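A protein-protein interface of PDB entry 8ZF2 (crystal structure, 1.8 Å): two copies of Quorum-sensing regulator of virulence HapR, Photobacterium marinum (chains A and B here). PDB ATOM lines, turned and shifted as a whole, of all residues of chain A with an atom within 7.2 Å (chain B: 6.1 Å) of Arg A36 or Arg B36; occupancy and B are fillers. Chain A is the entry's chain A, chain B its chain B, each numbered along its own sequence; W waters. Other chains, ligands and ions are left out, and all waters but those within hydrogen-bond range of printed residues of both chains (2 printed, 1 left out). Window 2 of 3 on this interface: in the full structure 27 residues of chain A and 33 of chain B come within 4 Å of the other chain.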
ATOM      1  N   VAL A  28      26.129  -6.410 -11.985  1.00  0.00           N
ATOM      2  CA  VAL A  28      25.651  -5.094 -11.575  1.00  0.00           C
ATOM      3  C   VAL A  28      26.470  -4.568 -10.402  1.00  0.00           C
ATOM      4  O   VAL A  28      26.666  -3.354 -10.272  1.00  0.00           O
ATOM      5  CB  VAL A  28      24.144  -5.133 -11.253  1.00  0.00           C
ATOM      6  CG1 VAL A  28      23.860  -6.026 -10.062  1.00  0.00           C
ATOM      7  CG2 VAL A  28      23.610  -3.723 -11.024  1.00  0.00           C
ATOM      8  N   PHE A  29      26.979  -5.459  -9.544  1.00  0.00           N
ATOM      9  CA  PHE A  29      27.861  -5.011  -8.469  1.00  0.00           C
ATOM     10  C   PHE A  29      29.109  -4.364  -9.046  1.00  0.00           C
ATOM     11  O   PHE A  29      29.592  -3.351  -8.526  1.00  0.00           O
ATOM     12  CB  PHE A  29      28.258  -6.184  -7.570  1.00  0.00           C
ATOM     13  CG  PHE A  29      27.161  -6.666  -6.660  1.00  0.00           C
ATOM     14  CD1 PHE A  29      25.888  -6.121  -6.721  1.00  0.00           C
ATOM     15  CD2 PHE A  29      27.406  -7.679  -5.743  1.00  0.00           C
ATOM     16  CE1 PHE A  29      24.881  -6.579  -5.887  1.00  0.00           C
ATOM     17  CE2 PHE A  29      26.404  -8.138  -4.906  1.00  0.00           C
ATOM     18  CZ  PHE A  29      25.141  -7.588  -4.981  1.00  0.00           C
ATOM     19  N   ARG A  32      27.800  -0.877 -10.742  1.00  0.00           N
ATOM     20  CA  ARG A  32      27.186   0.133  -9.891  1.00  0.00           C
ATOM     21  C   ARG A  32      27.690   0.136  -8.455  1.00  0.00           C
ATOM     22  O   ARG A  32      27.416   1.100  -7.730  1.00  0.00           O
ATOM     23  CB  ARG A  32      25.661  -0.050  -9.870  1.00  0.00           C
ATOM     24  CG  ARG A  32      24.981   0.115 -11.217  1.00  0.00           C
ATOM     25  CD  ARG A  32      23.633   0.804 -11.054  1.00  0.00           C
ATOM     26  NE  ARG A  32      22.567  -0.160 -10.804  1.00  0.00           N
ATOM     27  CZ  ARG A  32      21.676  -0.065  -9.826  1.00  0.00           C
ATOM     28  NH1 ARG A  32      21.692   0.944  -8.969  1.00  0.00           N
ATOM     29  NH2 ARG A  32      20.745  -1.007  -9.702  1.00  0.00           N
ATOM     30  N   GLY A  33      28.386  -0.898  -8.021  1.00  0.00           N
ATOM     31  CA  GLY A  33      28.817  -0.952  -6.640  1.00  0.00           C
ATOM     32  C   GLY A  33      28.161  -2.101  -5.885  1.00  0.00           C
ATOM     33  O   GLY A  33      27.020  -2.501  -6.164  1.00  0.00           O
ATOM     34  N   ILE A  34      28.894  -2.628  -4.896  1.00  0.00           N
ATOM     35  CA  ILE A  34      28.440  -3.796  -4.149  1.00  0.00           C
ATOM     36  C   ILE A  34      27.117  -3.504  -3.458  1.00  0.00           C
ATOM     37  O   ILE A  34      26.972  -2.506  -2.740  1.00  0.00           O
ATOM     38  CB  ILE A  34      29.521  -4.224  -3.145  1.00  0.00           C
ATOM     39  CG1 ILE A  34      30.771  -4.711  -3.884  1.00  0.00           C
ATOM     40  CG2 ILE A  34      28.995  -5.282  -2.193  1.00  0.00           C
ATOM     41  CD1 ILE A  34      31.961  -4.967  -2.973  1.00  0.00           C
ATOM     42  N   GLY A  35      26.133  -4.369  -3.695  1.00  0.00           N
ATOM     43  CA  GLY A  35      24.905  -4.353  -2.926  1.00  0.00           C
ATOM     44  C   GLY A  35      23.970  -3.202  -3.205  1.00  0.00           C
ATOM     45  O   GLY A  35      23.125  -2.890  -2.362  1.00  0.00           O
ATOM     46  N   ARG A  36      24.084  -2.559  -4.365  1.00  0.00           N
ATOM     47  CA  ARG A  36      23.214  -1.428  -4.663  1.00  0.00           C
ATOM     48  C   ARG A  36      21.982  -1.819  -5.468  1.00  0.00           C
ATOM     49  O   ARG A  36      20.967  -1.115  -5.399  1.00  0.00           O
ATOM     50  CB  ARG A  36      23.999  -0.335  -5.401  1.00  0.00           C
ATOM     51  CG  ARG A  36      25.247   0.121  -4.653  1.00  0.00           C
ATOM     52  CD  ARG A  36      25.715   1.501  -5.097  1.00  0.00           C
ATOM     53  NE  ARG A  36      26.803   2.008  -4.268  1.00  0.00           N
ATOM     54  CZ  ARG A  36      27.256   3.254  -4.309  1.00  0.00           C
ATOM     55  NH1 ARG A  36      26.739   4.151  -5.134  1.00  0.00           N
ATOM     56  NH2 ARG A  36      28.250   3.613  -3.498  1.00  0.00           N
ATOM     57  N   ALA A  37      22.035  -2.921  -6.208  1.00  0.00           N
ATOM     58  CA  ALA A  37      20.900  -3.367  -7.001  1.00  0.00           C
ATOM     59  C   ALA A  37      19.973  -4.246  -6.170  1.00  0.00           C
ATOM     60  O   ALA A  37      20.425  -5.077  -5.376  1.00  0.00           O
ATOM     61  CB  ALA A  37      21.371  -4.134  -8.236  1.00  0.00           C
ATOM     62  N   GLY A  38      18.672  -4.059  -6.363  1.00  0.00           N
ATOM     63  CA  GLY A  38      17.697  -4.869  -5.671  1.00  0.00           C
ATOM     64  C   GLY A  38      17.443  -6.193  -6.354  1.00  0.00           C
ATOM     65  O   GLY A  38      17.881  -6.446  -7.475  1.00  0.00           O
ATOM     66  N   ASP A  41      15.914  -5.647  -9.615  1.00  0.00           N
ATOM     67  CA  ASP A  41      16.846  -5.349 -10.696  1.00  0.00           C
ATOM     68  C   ASP A  41      17.428  -6.626 -11.287  1.00  0.00           C
ATOM     69  O   ASP A  41      17.499  -6.768 -12.513  1.00  0.00           O
ATOM     70  CB  ASP A  41      17.957  -4.425 -10.199  1.00  0.00           C
ATOM     71  CG  ASP A  41      17.418  -3.175  -9.532  1.00  0.00           C
ATOM     72  OD1 ASP A  41      16.516  -2.532 -10.115  1.00  0.00           O
ATOM     73  OD2 ASP A  41      17.894  -2.833  -8.428  1.00  0.00           O
ATOM     74  N   ARG A  60      18.365  -9.769   0.717  1.00  0.00           N
ATOM     75  CA  ARG A  60      19.369  -9.023  -0.032  1.00  0.00           C
ATOM     76  C   ARG A  60      20.771  -9.377   0.450  1.00  0.00           C
ATOM     77  O   ARG A  60      21.711  -9.476  -0.350  1.00  0.00           O
ATOM     78  CB  ARG A  60      19.113  -7.523   0.123  1.00  0.00           C
ATOM     79  CG  ARG A  60      20.319  -6.646  -0.145  1.00  0.00           C
ATOM     80  CD  ARG A  60      19.926  -5.174  -0.227  1.00  0.00           C
ATOM     81  NE  ARG A  60      18.984  -4.876  -1.301  1.00  0.00           N
ATOM     82  CZ  ARG A  60      19.049  -3.801  -2.076  1.00  0.00           C
ATOM     83  NH1 ARG A  60      20.070  -2.964  -2.016  1.00  0.00           N
ATOM     84  NH2 ARG A  60      18.056  -3.553  -2.923  1.00  0.00           N
ATOM     85  N   VAL A  64      24.336 -10.898  -1.424  1.00  0.00           N
ATOM     86  CA  VAL A  64      25.617 -10.198  -1.338  1.00  0.00           C
ATOM     87  C   VAL A  64      26.722 -11.153  -0.902  1.00  0.00           C
ATOM     88  O   VAL A  64      27.782 -11.233  -1.535  1.00  0.00           O
ATOM     89  CB  VAL A  64      25.508  -8.991  -0.389  1.00  0.00           C
ATOM     90  CG1 VAL A  64      26.895  -8.452  -0.050  1.00  0.00           C
ATOM     91  CG2 VAL A  64      24.659  -7.906  -1.020  1.00  0.00           C
ATOM     92  N   GLU A 117      36.867  -3.273  -4.600  1.00  0.00           N
ATOM     93  CA  GLU A 117      35.886  -2.428  -3.929  1.00  0.00           C
ATOM     94  C   GLU A 117      35.526  -2.998  -2.557  1.00  0.00           C
ATOM     95  O   GLU A 117      35.366  -2.252  -1.583  1.00  0.00           O
ATOM     96  CB  GLU A 117      34.644  -2.277  -4.807  1.00  0.00           C
ATOM     97  CG  GLU A 117      33.416  -1.839  -4.051  1.00  0.00           C
ATOM     98  CD  GLU A 117      32.204  -1.666  -4.944  1.00  0.00           C
ATOM     99  OE1 GLU A 117      32.275  -2.028  -6.141  1.00  0.00           O
ATOM    100  OE2 GLU A 117      31.177  -1.179  -4.435  1.00  0.00           O
ATOM    101  N   ASP A 124      31.203  -1.086   6.171  1.00  0.00           N
ATOM    102  CA  ASP A 124      30.057  -1.873   5.753  1.00  0.00           C
ATOM    103  C   ASP A 124      30.081  -3.227   6.448  1.00  0.00           C
ATOM    104  O   ASP A 124      31.140  -3.733   6.830  1.00  0.00           O
ATOM    105  CB  ASP A 124      30.061  -2.051   4.232  1.00  0.00           C
ATOM    106  CG  ASP A 124      28.780  -2.674   3.706  1.00  0.00           C
ATOM    107  OD1 ASP A 124      28.609  -3.908   3.820  1.00  0.00           O
ATOM    108  OD2 ASP A 124      27.941  -1.921   3.162  1.00  0.00           O
ATOM    109  N   VAL B  28      27.360  10.817   5.483  1.00  0.00           N
ATOM    110  CA  VAL B  28      26.550   9.689   5.034  1.00  0.00           C
ATOM    111  C   VAL B  28      27.280   8.896   3.954  1.00  0.00           C
ATOM    112  O   VAL B  28      27.134   7.670   3.873  1.00  0.00           O
ATOM    113  CB  VAL B  28      25.167  10.180   4.568  1.00  0.00           C
ATOM    114  CG1 VAL B  28      25.307  11.243   3.503  1.00  0.00           C
ATOM    115  CG2 VAL B  28      24.309   9.018   4.080  1.00  0.00           C
ATOM    116  N   PHE B  29      28.092   9.564   3.128  1.00  0.00           N
ATOM    117  CA  PHE B  29      28.916   8.844   2.161  1.00  0.00           C
ATOM    118  C   PHE B  29      29.858   7.876   2.867  1.00  0.00           C
ATOM    119  O   PHE B  29      30.016   6.725   2.447  1.00  0.00           O
ATOM    120  CB  PHE B  29      29.717   9.829   1.304  1.00  0.00           C
ATOM    121  CG  PHE B  29      28.913  10.490   0.219  1.00  0.00           C
ATOM    122  CD1 PHE B  29      27.534  10.351   0.174  1.00  0.00           C
ATOM    123  CD2 PHE B  29      29.539  11.246  -0.759  1.00  0.00           C
ATOM    124  CE1 PHE B  29      26.789  10.962  -0.820  1.00  0.00           C
ATOM    125  CE2 PHE B  29      28.802  11.857  -1.760  1.00  0.00           C
ATOM    126  CZ  PHE B  29      27.427  11.715  -1.789  1.00  0.00           C
ATOM    127  N   ARG B  32      27.450   5.011   4.417  1.00  0.00           N
ATOM    128  CA  ARG B  32      26.662   4.180   3.517  1.00  0.00           C
ATOM    129  C   ARG B  32      27.306   3.944   2.159  1.00  0.00           C
ATOM    130  O   ARG B  32      26.903   3.008   1.462  1.00  0.00           O
ATOM    131  CB  ARG B  32      25.272   4.797   3.300  1.00  0.00           C
ATOM    132  CG  ARG B  32      24.622   5.336   4.569  1.00  0.00           C
ATOM    133  CD  ARG B  32      23.121   5.067   4.594  1.00  0.00           C
ATOM    134  NE  ARG B  32      22.444   5.567   3.402  1.00  0.00           N
ATOM    135  CZ  ARG B  32      21.670   6.646   3.370  1.00  0.00           C
ATOM    136  NH1 ARG B  32      21.450   7.375   4.453  1.00  0.00           N
ATOM    137  NH2 ARG B  32      21.090   6.995   2.224  1.00  0.00           N
ATOM    138  N   GLY B  33      28.286   4.756   1.768  1.00  0.00           N
ATOM    139  CA  GLY B  33      28.900   4.628   0.462  1.00  0.00           C
ATOM    140  C   GLY B  33      28.756   5.891  -0.365  1.00  0.00           C
ATOM    141  O   GLY B  33      27.795   6.643  -0.184  1.00  0.00           O
ATOM    142  N   ILE B  34      29.709   6.131  -1.272  1.00  0.00           N
ATOM    143  CA  ILE B  34      29.670   7.320  -2.117  1.00  0.00           C
ATOM    144  C   ILE B  34      28.402   7.307  -2.952  1.00  0.00           C
ATOM    145  O   ILE B  34      28.091   6.313  -3.621  1.00  0.00           O
ATOM    146  CB  ILE B  34      30.911   7.381  -3.020  1.00  0.00           C
ATOM    147  CG1 ILE B  34      32.183   7.556  -2.190  1.00  0.00           C
ATOM    148  CG2 ILE B  34      30.778   8.509  -4.043  1.00  0.00           C
ATOM    149  CD1 ILE B  34      33.452   7.311  -2.986  1.00  0.00           C
ATOM    150  N   GLY B  35      27.661   8.409  -2.913  1.00  0.00           N
ATOM    151  CA  GLY B  35      26.472   8.553  -3.730  1.00  0.00           C
ATOM    152  C   GLY B  35      25.241   7.848  -3.212  1.00  0.00           C
ATOM    153  O   GLY B  35      24.258   7.736  -3.951  1.00  0.00           O
ATOM    154  N   ARG B  36      25.259   7.385  -1.962  1.00  0.00           N
ATOM    155  CA  ARG B  36      24.166   6.625  -1.369  1.00  0.00           C
ATOM    156  C   ARG B  36      23.225   7.489  -0.538  1.00  0.00           C
ATOM    157  O   ARG B  36      22.518   6.967   0.330  1.00  0.00           O
ATOM    158  CB  ARG B  36      24.728   5.494  -0.511  1.00  0.00           C
ATOM    159  CG  ARG B  36      25.468   4.442  -1.303  1.00  0.00           C
ATOM    160  CD  ARG B  36      24.562   3.829  -2.345  1.00  0.00           C
ATOM    161  NE  ARG B  36      23.426   3.152  -1.727  1.00  0.00           N
ATOM    162  CZ  ARG B  36      23.424   1.874  -1.375  1.00  0.00           C
ATOM    163  NH1 ARG B  36      24.493   1.111  -1.538  1.00  0.00           N
ATOM    164  NH2 ARG B  36      22.326   1.349  -0.839  1.00  0.00           N
ATOM    165  N   ALA B  37      23.205   8.794  -0.776  1.00  0.00           N
ATOM    166  CA  ALA B  37      22.262   9.676  -0.106  1.00  0.00           C
ATOM    167  C   ALA B  37      21.683  10.636  -1.128  1.00  0.00           C
ATOM    168  O   ALA B  37      22.430  11.256  -1.890  1.00  0.00           O
ATOM    169  CB  ALA B  37      22.927  10.458   1.029  1.00  0.00           C
ATOM    170  N   GLY B  38      20.358  10.751  -1.144  1.00  0.00           N
ATOM    171  CA  GLY B  38      19.710  11.726  -1.991  1.00  0.00           C
ATOM    172  C   GLY B  38      19.622  13.086  -1.327  1.00  0.00           C
ATOM    173  O   GLY B  38      19.984  13.275  -0.165  1.00  0.00           O
ATOM    174  N   ASP B  41      17.514  13.129   1.863  1.00  0.00           N
ATOM    175  CA  ASP B  41      18.197  12.673   3.069  1.00  0.00           C
ATOM    176  C   ASP B  41      19.044  13.785   3.674  1.00  0.00           C
ATOM    177  O   ASP B  41      19.029  13.996   4.891  1.00  0.00           O
ATOM    178  CB  ASP B  41      19.070  11.456   2.759  1.00  0.00           C
ATOM    179  CG  ASP B  41      18.296  10.331   2.109  1.00  0.00           C
ATOM    180  OD1 ASP B  41      17.209   9.984   2.622  1.00  0.00           O
ATOM    181  OD2 ASP B  41      18.779   9.792   1.087  1.00  0.00           O
ATOM    182  N   ARG B  60      22.269  15.369  -8.180  1.00  0.00           N
ATOM    183  CA  ARG B  60      22.990  14.466  -7.288  1.00  0.00           C
ATOM    184  C   ARG B  60      24.454  14.348  -7.688  1.00  0.00           C
ATOM    185  O   ARG B  60      25.323  14.176  -6.826  1.00  0.00           O
ATOM    186  CB  ARG B  60      22.339  13.083  -7.286  1.00  0.00           C
ATOM    187  CG  ARG B  60      20.971  13.040  -6.628  1.00  0.00           C
ATOM    188  CD  ARG B  60      20.345  11.655  -6.720  1.00  0.00           C
ATOM    189  NE  ARG B  60      20.656  10.823  -5.561  1.00  0.00           N
ATOM    190  CZ  ARG B  60      21.308   9.669  -5.619  1.00  0.00           C
ATOM    191  NH1 ARG B  60      21.748   9.180  -6.767  1.00  0.00           N
ATOM    192  NH2 ARG B  60      21.516   8.984  -4.498  1.00  0.00           N
ATOM    193  N   VAL B  64      27.855  14.840  -5.327  1.00  0.00           N
ATOM    194  CA  VAL B  64      28.901  13.822  -5.249  1.00  0.00           C
ATOM    195  C   VAL B  64      30.244  14.407  -5.671  1.00  0.00           C
ATOM    196  O   VAL B  64      31.263  14.229  -4.990  1.00  0.00           O
ATOM    197  CB  VAL B  64      28.529  12.599  -6.107  1.00  0.00           C
ATOM    198  CG1 VAL B  64      29.744  11.685  -6.286  1.00  0.00           C
ATOM    199  CG2 VAL B  64      27.374  11.833  -5.477  1.00  0.00           C
ATOM    200  N   GLU B 117      37.742   4.399  -0.648  1.00  0.00           N
ATOM    201  CA  GLU B 117      36.599   3.843  -1.365  1.00  0.00           C
ATOM    202  C   GLU B 117      36.521   4.403  -2.778  1.00  0.00           C
ATOM    203  O   GLU B 117      36.283   3.665  -3.746  1.00  0.00           O
ATOM    204  CB  GLU B 117      35.317   4.142  -0.589  1.00  0.00           C
ATOM    205  CG  GLU B 117      34.050   3.896  -1.364  1.00  0.00           C
ATOM    206  CD  GLU B 117      32.824   4.439  -0.649  1.00  0.00           C
ATOM    207  OE1 GLU B 117      32.979   5.099   0.407  1.00  0.00           O
ATOM    208  OE2 GLU B 117      31.710   4.201  -1.146  1.00  0.00           O
ATOM    209  N   ARG B 123      34.143   3.506 -11.791  1.00  0.00           N
ATOM    210  CA  ARG B 123      32.851   3.684 -12.438  1.00  0.00           C
ATOM    211  C   ARG B 123      32.690   5.132 -12.878  1.00  0.00           C
ATOM    212  O   ARG B 123      33.469   6.010 -12.498  1.00  0.00           O
ATOM    213  CB  ARG B 123      31.699   3.304 -11.503  1.00  0.00           C
ATOM    214  CG  ARG B 123      31.237   4.460 -10.620  1.00  0.00           C
ATOM    215  CD  ARG B 123      30.097   4.068  -9.695  1.00  0.00           C
ATOM    216  NE  ARG B 123      30.519   3.033  -8.761  1.00  0.00           N
ATOM    217  CZ  ARG B 123      30.524   3.174  -7.442  1.00  0.00           C
ATOM    218  NH1 ARG B 123      30.097   4.284  -6.863  1.00  0.00           N
ATOM    219  NH2 ARG B 123      30.980   2.180  -6.687  1.00  0.00           N
HETATM  220  O   HOH W   1      30.403   2.013  -1.584  1.00  0.00           O
HETATM  221  O   HOH W   2      31.588   3.859  -4.017  1.00  0.00           O
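O of Ile B34 is in hydrogen-bond range of NH2 of Arg A36 (2.7 Å).
Along chain A the printed residues that touch a printed residue of chain B span positions 32 to 36. Printed residues of chain B that touch a printed residue of chain A: Gly B33, Ile B34, Arg B36 and Arg B123. Among the printed residues, 6 pairs touch across the chains. Among the printed residues, no Asp or Glu carboxylate lies within 4 Å of a Lys or Arg side-chain nitrogen of the other chain.
Arg A36 touches Gly B33, but with the chains exchanged Gly A33 does not touch Arg B36 (6.4 Å). Arg A36 touches Ile B34, but with the chains exchanged Ile A34 does not touch Arg B36 (4.5 Å). Arg A36 touches its own counterpart, Arg B36. 13 positions are printed for both chains. Of the 6 pairs that touch across the chains among the printed residues, 1 has its exchanged pair printed and touching as well.
Water W1 lies within hydrogen-bond range of the side-chain carboxylate (OE2) of Glu B117 (2.6 Å) and the guanidinium group (NH2) of Arg A36 (3.3 Å). Water W2 lies within hydrogen-bond range of OE2 of Glu B117, NH2 of Arg B123 and NH2 of Arg A36.
The guanidinium group (NE) of Arg B32 lies close to the backbone carbonyl oxygen (O) of Arg B36 (3.4 Å). OD2 of Asp A41 is in salt-bridge range of NH2 of Arg A32 (3.6 Å). OE2 of Glu B117 lies within hydrogen-bond range of N of Ile B34 (2.8 Å).
Of chain B, only Gly B33 (3.9 Å), Ile B34 (2.7 Å), Arg B36 (3.4 Å) and Arg B123 (3.8 Å) come within 4 Å of Arg A36. Arg B36 touches just one residue of chain A: Arg A36. No residue of chain A comes within 4 Å of Gly B35. Of the printed residues of chain A, Ile B34 touches Arg A36. Of the printed residues of chain A, Arg B123 touches Arg A32 (3.7 Å), Gly A33 (3.8 Å) and Arg A36 (3.8 Å). Printed residues of chain B within 4 Å of Arg A32: Arg B123. Of the printed residues of chain B, Gly A33 touches Arg B123 (3.8 Å). Arg B32 touches none of the printed residues of chain A. The nearest residue of chain A that does not touch Arg B36 is Gly A35 (4.3 Å).
Among the printed residues, pairs that only touch across the chains: Arg A36 with Arg B36 (3.4 Å), Arg A32 with Arg B123 (3.7 Å), Arg A36 with Arg B123 (3.8 Å), Gly A33 with Arg B123 (3.8 Å) and Arg A36 with Gly B33 (3.9 Å).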
